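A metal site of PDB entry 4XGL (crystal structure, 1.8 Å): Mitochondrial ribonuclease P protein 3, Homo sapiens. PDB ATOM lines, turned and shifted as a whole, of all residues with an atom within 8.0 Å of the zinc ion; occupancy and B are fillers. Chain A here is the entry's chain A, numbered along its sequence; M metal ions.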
ATOM      1  N   LYS A 132      -6.606  -0.793 -34.974  1.00  0.00           N
ATOM      2  CA  LYS A 132      -6.757   0.447 -34.219  1.00  0.00           C
ATOM      3  C   LYS A 132      -6.864   0.124 -32.733  1.00  0.00           C
ATOM      4  O   LYS A 132      -7.644  -0.735 -32.340  1.00  0.00           O
ATOM      5  CB  LYS A 132      -7.984   1.228 -34.693  1.00  0.00           C
ATOM      6  CG  LYS A 132      -8.336   2.408 -33.802  1.00  0.00           C
ATOM      7  CD  LYS A 132      -9.685   3.012 -34.190  1.00  0.00           C
ATOM      8  CE  LYS A 132     -10.079   4.135 -33.235  1.00  0.00           C
ATOM      9  NZ  LYS A 132     -11.444   4.663 -33.526  1.00  0.00           N
ATOM     10  N   GLN A 134      -7.419   1.396 -28.632  1.00  0.00           N
ATOM     11  CA  GLN A 134      -8.042   2.405 -27.769  1.00  0.00           C
ATOM     12  C   GLN A 134      -7.964   1.916 -26.328  1.00  0.00           C
ATOM     13  O   GLN A 134      -8.053   0.705 -26.069  1.00  0.00           O
ATOM     14  CB  GLN A 134      -9.497   2.638 -28.148  1.00  0.00           C
ATOM     15  CG  GLN A 134      -9.743   3.390 -29.428  1.00  0.00           C
ATOM     16  CD  GLN A 134     -11.182   3.885 -29.493  1.00  0.00           C
ATOM     17  OE1 GLN A 134     -12.124   3.103 -29.410  1.00  0.00           O
ATOM     18  NE2 GLN A 134     -11.353   5.193 -29.613  1.00  0.00           N
ATOM     19  N   THR A 136      -9.743   1.552 -22.884  1.00  0.00           N
ATOM     20  CA  THR A 136     -11.168   1.454 -22.590  1.00  0.00           C
ATOM     21  C   THR A 136     -11.437   0.883 -21.193  1.00  0.00           C
ATOM     22  O   THR A 136     -10.507   0.546 -20.453  1.00  0.00           O
ATOM     23  CB  THR A 136     -11.897   0.526 -23.607  1.00  0.00           C
ATOM     24  OG1 THR A 136     -11.454  -0.826 -23.421  1.00  0.00           O
ATOM     25  CG2 THR A 136     -11.613   0.944 -25.039  1.00  0.00           C
ATOM     26  N   THR A 137     -12.718   0.800 -20.853  1.00  0.00           N
ATOM     27  CA  THR A 137     -13.172   0.043 -19.700  1.00  0.00           C
ATOM     28  C   THR A 137     -14.215  -0.931 -20.190  1.00  0.00           C
ATOM     29  O   THR A 137     -14.568  -0.910 -21.372  1.00  0.00           O
ATOM     30  CB  THR A 137     -13.779   0.943 -18.605  1.00  0.00           C
ATOM     31  OG1 THR A 137     -14.977   1.546 -19.085  1.00  0.00           O
ATOM     32  CG2 THR A 137     -12.793   2.015 -18.187  1.00  0.00           C
ATOM     33  N   VAL A 138     -14.725  -1.776 -19.317  1.00  0.00           N
ATOM     34  CA  VAL A 138     -15.795  -2.670 -19.711  1.00  0.00           C
ATOM     35  C   VAL A 138     -17.046  -2.278 -18.929  1.00  0.00           C
ATOM     36  O   VAL A 138     -16.982  -2.061 -17.736  1.00  0.00           O
ATOM     37  CB  VAL A 138     -15.445  -4.157 -19.448  1.00  0.00           C
ATOM     38  CG1 VAL A 138     -16.630  -5.058 -19.757  1.00  0.00           C
ATOM     39  CG2 VAL A 138     -14.194  -4.581 -20.260  1.00  0.00           C
ATOM     40  N   GLN A 143     -19.789  -5.499 -22.076  1.00  0.00           N
ATOM     41  CA  GLN A 143     -19.498  -4.904 -23.373  1.00  0.00           C
ATOM     42  C   GLN A 143     -18.325  -3.932 -23.260  1.00  0.00           C
ATOM     43  O   GLN A 143     -18.311  -3.060 -22.379  1.00  0.00           O
ATOM     44  CB  GLN A 143     -20.738  -4.194 -23.912  1.00  0.00           C
ATOM     45  CG  GLN A 143     -21.865  -5.137 -24.304  1.00  0.00           C
ATOM     46  CD  GLN A 143     -23.208  -4.437 -24.399  1.00  0.00           C
ATOM     47  OE1 GLN A 143     -23.472  -3.461 -23.690  1.00  0.00           O
ATOM     48  NE2 GLN A 143     -24.077  -4.946 -25.277  1.00  0.00           N
ATOM     49  N   CYS A 144     -17.348  -4.091 -24.139  1.00  0.00           N
ATOM     50  CA  CYS A 144     -16.232  -3.164 -24.161  1.00  0.00           C
ATOM     51  C   CYS A 144     -16.742  -1.756 -24.477  1.00  0.00           C
ATOM     52  O   CYS A 144     -17.528  -1.557 -25.403  1.00  0.00           O
ATOM     53  CB  CYS A 144     -15.175  -3.580 -25.200  1.00  0.00           C
ATOM     54  SG  CYS A 144     -13.923  -2.330 -25.413  1.00  0.00           S
ATOM     55  N   SER A 145     -16.269  -0.774 -23.705  1.00  0.00           N
ATOM     56  CA  SER A 145     -16.720   0.608 -23.879  1.00  0.00           C
ATOM     57  C   SER A 145     -16.199   1.223 -25.165  1.00  0.00           C
ATOM     58  O   SER A 145     -16.656   2.287 -25.582  1.00  0.00           O
ATOM     59  CB  SER A 145     -16.298   1.465 -22.678  1.00  0.00           C
ATOM     60  OG  SER A 145     -14.900   1.673 -22.686  1.00  0.00           O
ATOM     61  N   GLY A 146     -15.221   0.566 -25.792  1.00  0.00           N
ATOM     62  CA  GLY A 146     -14.725   1.018 -27.068  1.00  0.00           C
ATOM     63  C   GLY A 146     -15.501   0.483 -28.266  1.00  0.00           C
ATOM     64  O   GLY A 146     -16.119   1.239 -28.994  1.00  0.00           O
ATOM     65  N   CYS A 147     -15.484  -0.839 -28.449  1.00  0.00           N
ATOM     66  CA  CYS A 147     -15.986  -1.438 -29.683  1.00  0.00           C
ATOM     67  C   CYS A 147     -17.346  -2.113 -29.538  1.00  0.00           C
ATOM     68  O   CYS A 147     -17.940  -2.531 -30.538  1.00  0.00           O
ATOM     69  CB  CYS A 147     -14.972  -2.448 -30.230  1.00  0.00           C
ATOM     70  SG  CYS A 147     -14.884  -3.998 -29.262  1.00  0.00           S
ATOM     71  N   GLY A 148     -17.846  -2.236 -28.310  1.00  0.00           N
ATOM     72  CA  GLY A 148     -19.152  -2.847 -28.099  1.00  0.00           C
ATOM     73  C   GLY A 148     -19.175  -4.363 -28.100  1.00  0.00           C
ATOM     74  O   GLY A 148     -20.223  -4.945 -27.871  1.00  0.00           O
ATOM     75  N   LYS A 149     -18.042  -5.004 -28.345  1.00  0.00           N
ATOM     76  CA  LYS A 149     -17.991  -6.471 -28.301  1.00  0.00           C
ATOM     77  C   LYS A 149     -18.160  -6.959 -26.888  1.00  0.00           C
ATOM     78  O   LYS A 149     -17.759  -6.293 -25.939  1.00  0.00           O
ATOM     79  CB  LYS A 149     -16.664  -7.008 -28.867  1.00  0.00           C
ATOM     80  CG  LYS A 149     -16.566  -7.043 -30.374  1.00  0.00           C
ATOM     81  CD  LYS A 149     -15.193  -7.565 -30.794  1.00  0.00           C
ATOM     82  CE  LYS A 149     -15.052  -7.656 -32.306  1.00  0.00           C
ATOM     83  NZ  LYS A 149     -15.639  -8.914 -32.847  1.00  0.00           N
ATOM     84  N   THR A 150     -18.761  -8.140 -26.735  1.00  0.00           N
ATOM     85  CA  THR A 150     -18.886  -8.738 -25.412  1.00  0.00           C
ATOM     86  C   THR A 150     -17.611  -9.468 -25.004  1.00  0.00           C
ATOM     87  O   THR A 150     -17.089 -10.289 -25.755  1.00  0.00           O
ATOM     88  CB  THR A 150     -20.074  -9.712 -25.358  1.00  0.00           C
ATOM     89  OG1 THR A 150     -21.273  -8.990 -25.669  1.00  0.00           O
ATOM     90  CG2 THR A 150     -20.194 -10.324 -23.979  1.00  0.00           C
ATOM     91  N   ILE A 151     -17.112  -9.145 -23.815  1.00  0.00           N
ATOM     92  CA  ILE A 151     -15.934  -9.791 -23.262  1.00  0.00           C
ATOM     93  C   ILE A 151     -16.256 -11.243 -22.895  1.00  0.00           C
ATOM     94  O   ILE A 151     -17.384 -11.541 -22.463  1.00  0.00           O
ATOM     95  CB  ILE A 151     -15.410  -9.012 -22.015  1.00  0.00           C
ATOM     96  CG1 ILE A 151     -14.988  -7.594 -22.386  1.00  0.00           C
ATOM     97  CG2 ILE A 151     -14.275  -9.743 -21.327  1.00  0.00           C
ATOM     98  CD1 ILE A 151     -13.822  -7.520 -23.382  1.00  0.00           C
ATOM     99  N   SER A 351      -9.969  -9.119 -33.252  1.00  0.00           N
ATOM    100  CA  SER A 351      -9.854  -8.204 -32.123  1.00  0.00           C
ATOM    101  C   SER A 351      -9.028  -8.807 -30.999  1.00  0.00           C
ATOM    102  O   SER A 351      -8.925 -10.023 -30.876  1.00  0.00           O
ATOM    103  CB  SER A 351     -11.236  -7.807 -31.603  1.00  0.00           C
ATOM    104  OG  SER A 351     -11.797  -8.830 -30.783  1.00  0.00           O
ATOM    105  N   TRP A 352      -8.448  -7.940 -30.181  1.00  0.00           N
ATOM    106  CA  TRP A 352      -7.814  -8.332 -28.923  1.00  0.00           C
ATOM    107  C   TRP A 352      -8.371  -7.465 -27.804  1.00  0.00           C
ATOM    108  O   TRP A 352      -8.677  -6.298 -28.019  1.00  0.00           O
ATOM    109  CB  TRP A 352      -6.281  -8.184 -28.972  1.00  0.00           C
ATOM    110  CG  TRP A 352      -5.587  -9.259 -29.740  1.00  0.00           C
ATOM    111  CD1 TRP A 352      -5.364  -9.296 -31.086  1.00  0.00           C
ATOM    112  CD2 TRP A 352      -4.996 -10.456 -29.196  1.00  0.00           C
ATOM    113  NE1 TRP A 352      -4.686 -10.453 -31.425  1.00  0.00           N
ATOM    114  CE2 TRP A 352      -4.447 -11.178 -30.281  1.00  0.00           C
ATOM    115  CE3 TRP A 352      -4.886 -10.989 -27.904  1.00  0.00           C
ATOM    116  CZ2 TRP A 352      -3.791 -12.407 -30.110  1.00  0.00           C
ATOM    117  CZ3 TRP A 352      -4.228 -12.227 -27.744  1.00  0.00           C
ATOM    118  CH2 TRP A 352      -3.704 -12.913 -28.832  1.00  0.00           C
ATOM    119  N   HIS A 353      -8.520  -8.035 -26.620  1.00  0.00           N
ATOM    120  CA  HIS A 353      -8.780  -7.200 -25.452  1.00  0.00           C
ATOM    121  C   HIS A 353      -7.800  -7.590 -24.356  1.00  0.00           C
ATOM    122  O   HIS A 353      -7.698  -8.748 -23.966  1.00  0.00           O
ATOM    123  CB  HIS A 353     -10.247  -7.332 -25.006  1.00  0.00           C
ATOM    124  CG  HIS A 353     -11.210  -6.714 -25.967  1.00  0.00           C
ATOM    125  ND1 HIS A 353     -11.622  -7.359 -27.118  1.00  0.00           N
ATOM    126  CD2 HIS A 353     -11.810  -5.502 -25.984  1.00  0.00           C
ATOM    127  CE1 HIS A 353     -12.447  -6.570 -27.785  1.00  0.00           C
ATOM    128  NE2 HIS A 353     -12.589  -5.446 -27.113  1.00  0.00           N
ATOM    129  N   ILE A 354      -7.069  -6.594 -23.884  1.00  0.00           N
ATOM    130  CA  ILE A 354      -5.924  -6.810 -23.034  1.00  0.00           C
ATOM    131  C   ILE A 354      -6.032  -5.955 -21.778  1.00  0.00           C
ATOM    132  O   ILE A 354      -5.812  -4.741 -21.834  1.00  0.00           O
ATOM    133  CB  ILE A 354      -4.614  -6.481 -23.807  1.00  0.00           C
ATOM    134  CG1 ILE A 354      -4.445  -7.408 -25.018  1.00  0.00           C
ATOM    135  CG2 ILE A 354      -3.399  -6.574 -22.894  1.00  0.00           C
ATOM    136  CD1 ILE A 354      -3.272  -7.015 -25.965  1.00  0.00           C
ATOM    137  N   TRP A 372      -8.548  -1.572 -19.824  1.00  0.00           N
ATOM    138  CA  TRP A 372      -8.334  -2.480 -20.937  1.00  0.00           C
ATOM    139  C   TRP A 372      -7.753  -1.779 -22.162  1.00  0.00           C
ATOM    140  O   TRP A 372      -8.054  -0.609 -22.414  1.00  0.00           O
ATOM    141  CB  TRP A 372      -9.648  -3.158 -21.340  1.00  0.00           C
ATOM    142  CG  TRP A 372     -10.256  -4.133 -20.341  1.00  0.00           C
ATOM    143  CD1 TRP A 372     -10.835  -3.834 -19.144  1.00  0.00           C
ATOM    144  CD2 TRP A 372     -10.369  -5.553 -20.489  1.00  0.00           C
ATOM    145  NE1 TRP A 372     -11.292  -4.969 -18.527  1.00  0.00           N
ATOM    146  CE2 TRP A 372     -11.029  -6.049 -19.337  1.00  0.00           C
ATOM    147  CE3 TRP A 372      -9.978  -6.472 -21.478  1.00  0.00           C
ATOM    148  CZ2 TRP A 372     -11.292  -7.405 -19.139  1.00  0.00           C
ATOM    149  CZ3 TRP A 372     -10.258  -7.829 -21.282  1.00  0.00           C
ATOM    150  CH2 TRP A 372     -10.903  -8.274 -20.121  1.00  0.00           C
ATOM    151  N   LEU A 373      -6.915  -2.488 -22.914  1.00  0.00           N
ATOM    152  CA  LEU A 373      -6.552  -2.082 -24.272  1.00  0.00           C
ATOM    153  C   LEU A 373      -7.449  -2.844 -25.242  1.00  0.00           C
ATOM    154  O   LEU A 373      -7.491  -4.084 -25.255  1.00  0.00           O
ATOM    155  CB  LEU A 373      -5.066  -2.350 -24.544  1.00  0.00           C
ATOM    156  CG  LEU A 373      -4.594  -2.282 -26.001  1.00  0.00           C
ATOM    157  CD1 LEU A 373      -4.831  -0.856 -26.591  1.00  0.00           C
ATOM    158  CD2 LEU A 373      -3.116  -2.650 -26.086  1.00  0.00           C
ATOM    159  N   CYS A 374      -8.203  -2.083 -26.046  1.00  0.00           N
ATOM    160  CA  CYS A 374      -9.107  -2.629 -27.060  1.00  0.00           C
ATOM    161  C   CYS A 374      -8.484  -2.471 -28.438  1.00  0.00           C
ATOM    162  O   CYS A 374      -8.140  -1.351 -28.857  1.00  0.00           O
ATOM    163  CB  CYS A 374     -10.479  -1.922 -27.015  1.00  0.00           C
ATOM    164  SG  CYS A 374     -11.434  -2.084 -28.549  1.00  0.00           S
ATOM    165  N   LEU A 375      -8.311  -3.589 -29.127  1.00  0.00           N
ATOM    166  CA  LEU A 375      -7.680  -3.567 -30.447  1.00  0.00           C
ATOM    167  C   LEU A 375      -8.649  -4.195 -31.428  1.00  0.00           C
ATOM    168  O   LEU A 375      -9.197  -5.257 -31.170  1.00  0.00           O
ATOM    169  CB  LEU A 375      -6.357  -4.328 -30.460  1.00  0.00           C
ATOM    170  CG  LEU A 375      -5.197  -3.628 -29.760  1.00  0.00           C
ATOM    171  CD1 LEU A 375      -4.204  -4.668 -29.210  1.00  0.00           C
ATOM    172  CD2 LEU A 375      -4.502  -2.632 -30.717  1.00  0.00           C
ATOM    173  N   HIS A 376      -8.880  -3.502 -32.538  1.00  0.00           N
ATOM    174  CA  HIS A 376      -9.803  -4.012 -33.547  1.00  0.00           C
ATOM    175  C   HIS A 376      -9.300  -3.665 -34.939  1.00  0.00           C
ATOM    176  O   HIS A 376      -8.591  -2.678 -35.127  1.00  0.00           O
ATOM    177  CB  HIS A 376     -11.227  -3.450 -33.331  1.00  0.00           C
ATOM    178  CG  HIS A 376     -11.331  -1.968 -33.553  1.00  0.00           C
ATOM    179  ND1 HIS A 376     -11.642  -1.417 -34.775  1.00  0.00           N
ATOM    180  CD2 HIS A 376     -11.167  -0.926 -32.704  1.00  0.00           C
ATOM    181  CE1 HIS A 376     -11.672  -0.105 -34.675  1.00  0.00           C
ATOM    182  NE2 HIS A 376     -11.380   0.222 -33.422  1.00  0.00           N
HETATM  183 ZN    ZN M   1     -13.196  -3.402 -27.646  1.00  0.00          ZN
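The backbone carbonyl oxygen of Gln 134 is in hydrogen-bond range of the backbone NH of Cys 374. The backbone NH of Lys 149 lies close to the side-chain sulfur of Cys 147 (3.4 Å). SG of Cys 144 sits close to N of Gly 146 (3.2 Å). O of Lys 149 lies within hydrogen-bond range of N of Cys 144, at 2.9 Å. SG of Cys 144 sits close to OG1 of Thr 136 (3.5 Å).
Of the 23 residues printed, 4 come within 4 Å of the zinc ion.
The zinc ion is bound by NE2 of His 353. SG of Cys 374 binds the zinc ion (2.4 Å). SG of Cys 147 binds the zinc ion (2.4 Å). The side-chain sulfur (SG) of Cys 144 binds the zinc ion. The zinc ion has four donor atoms within binding distance.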
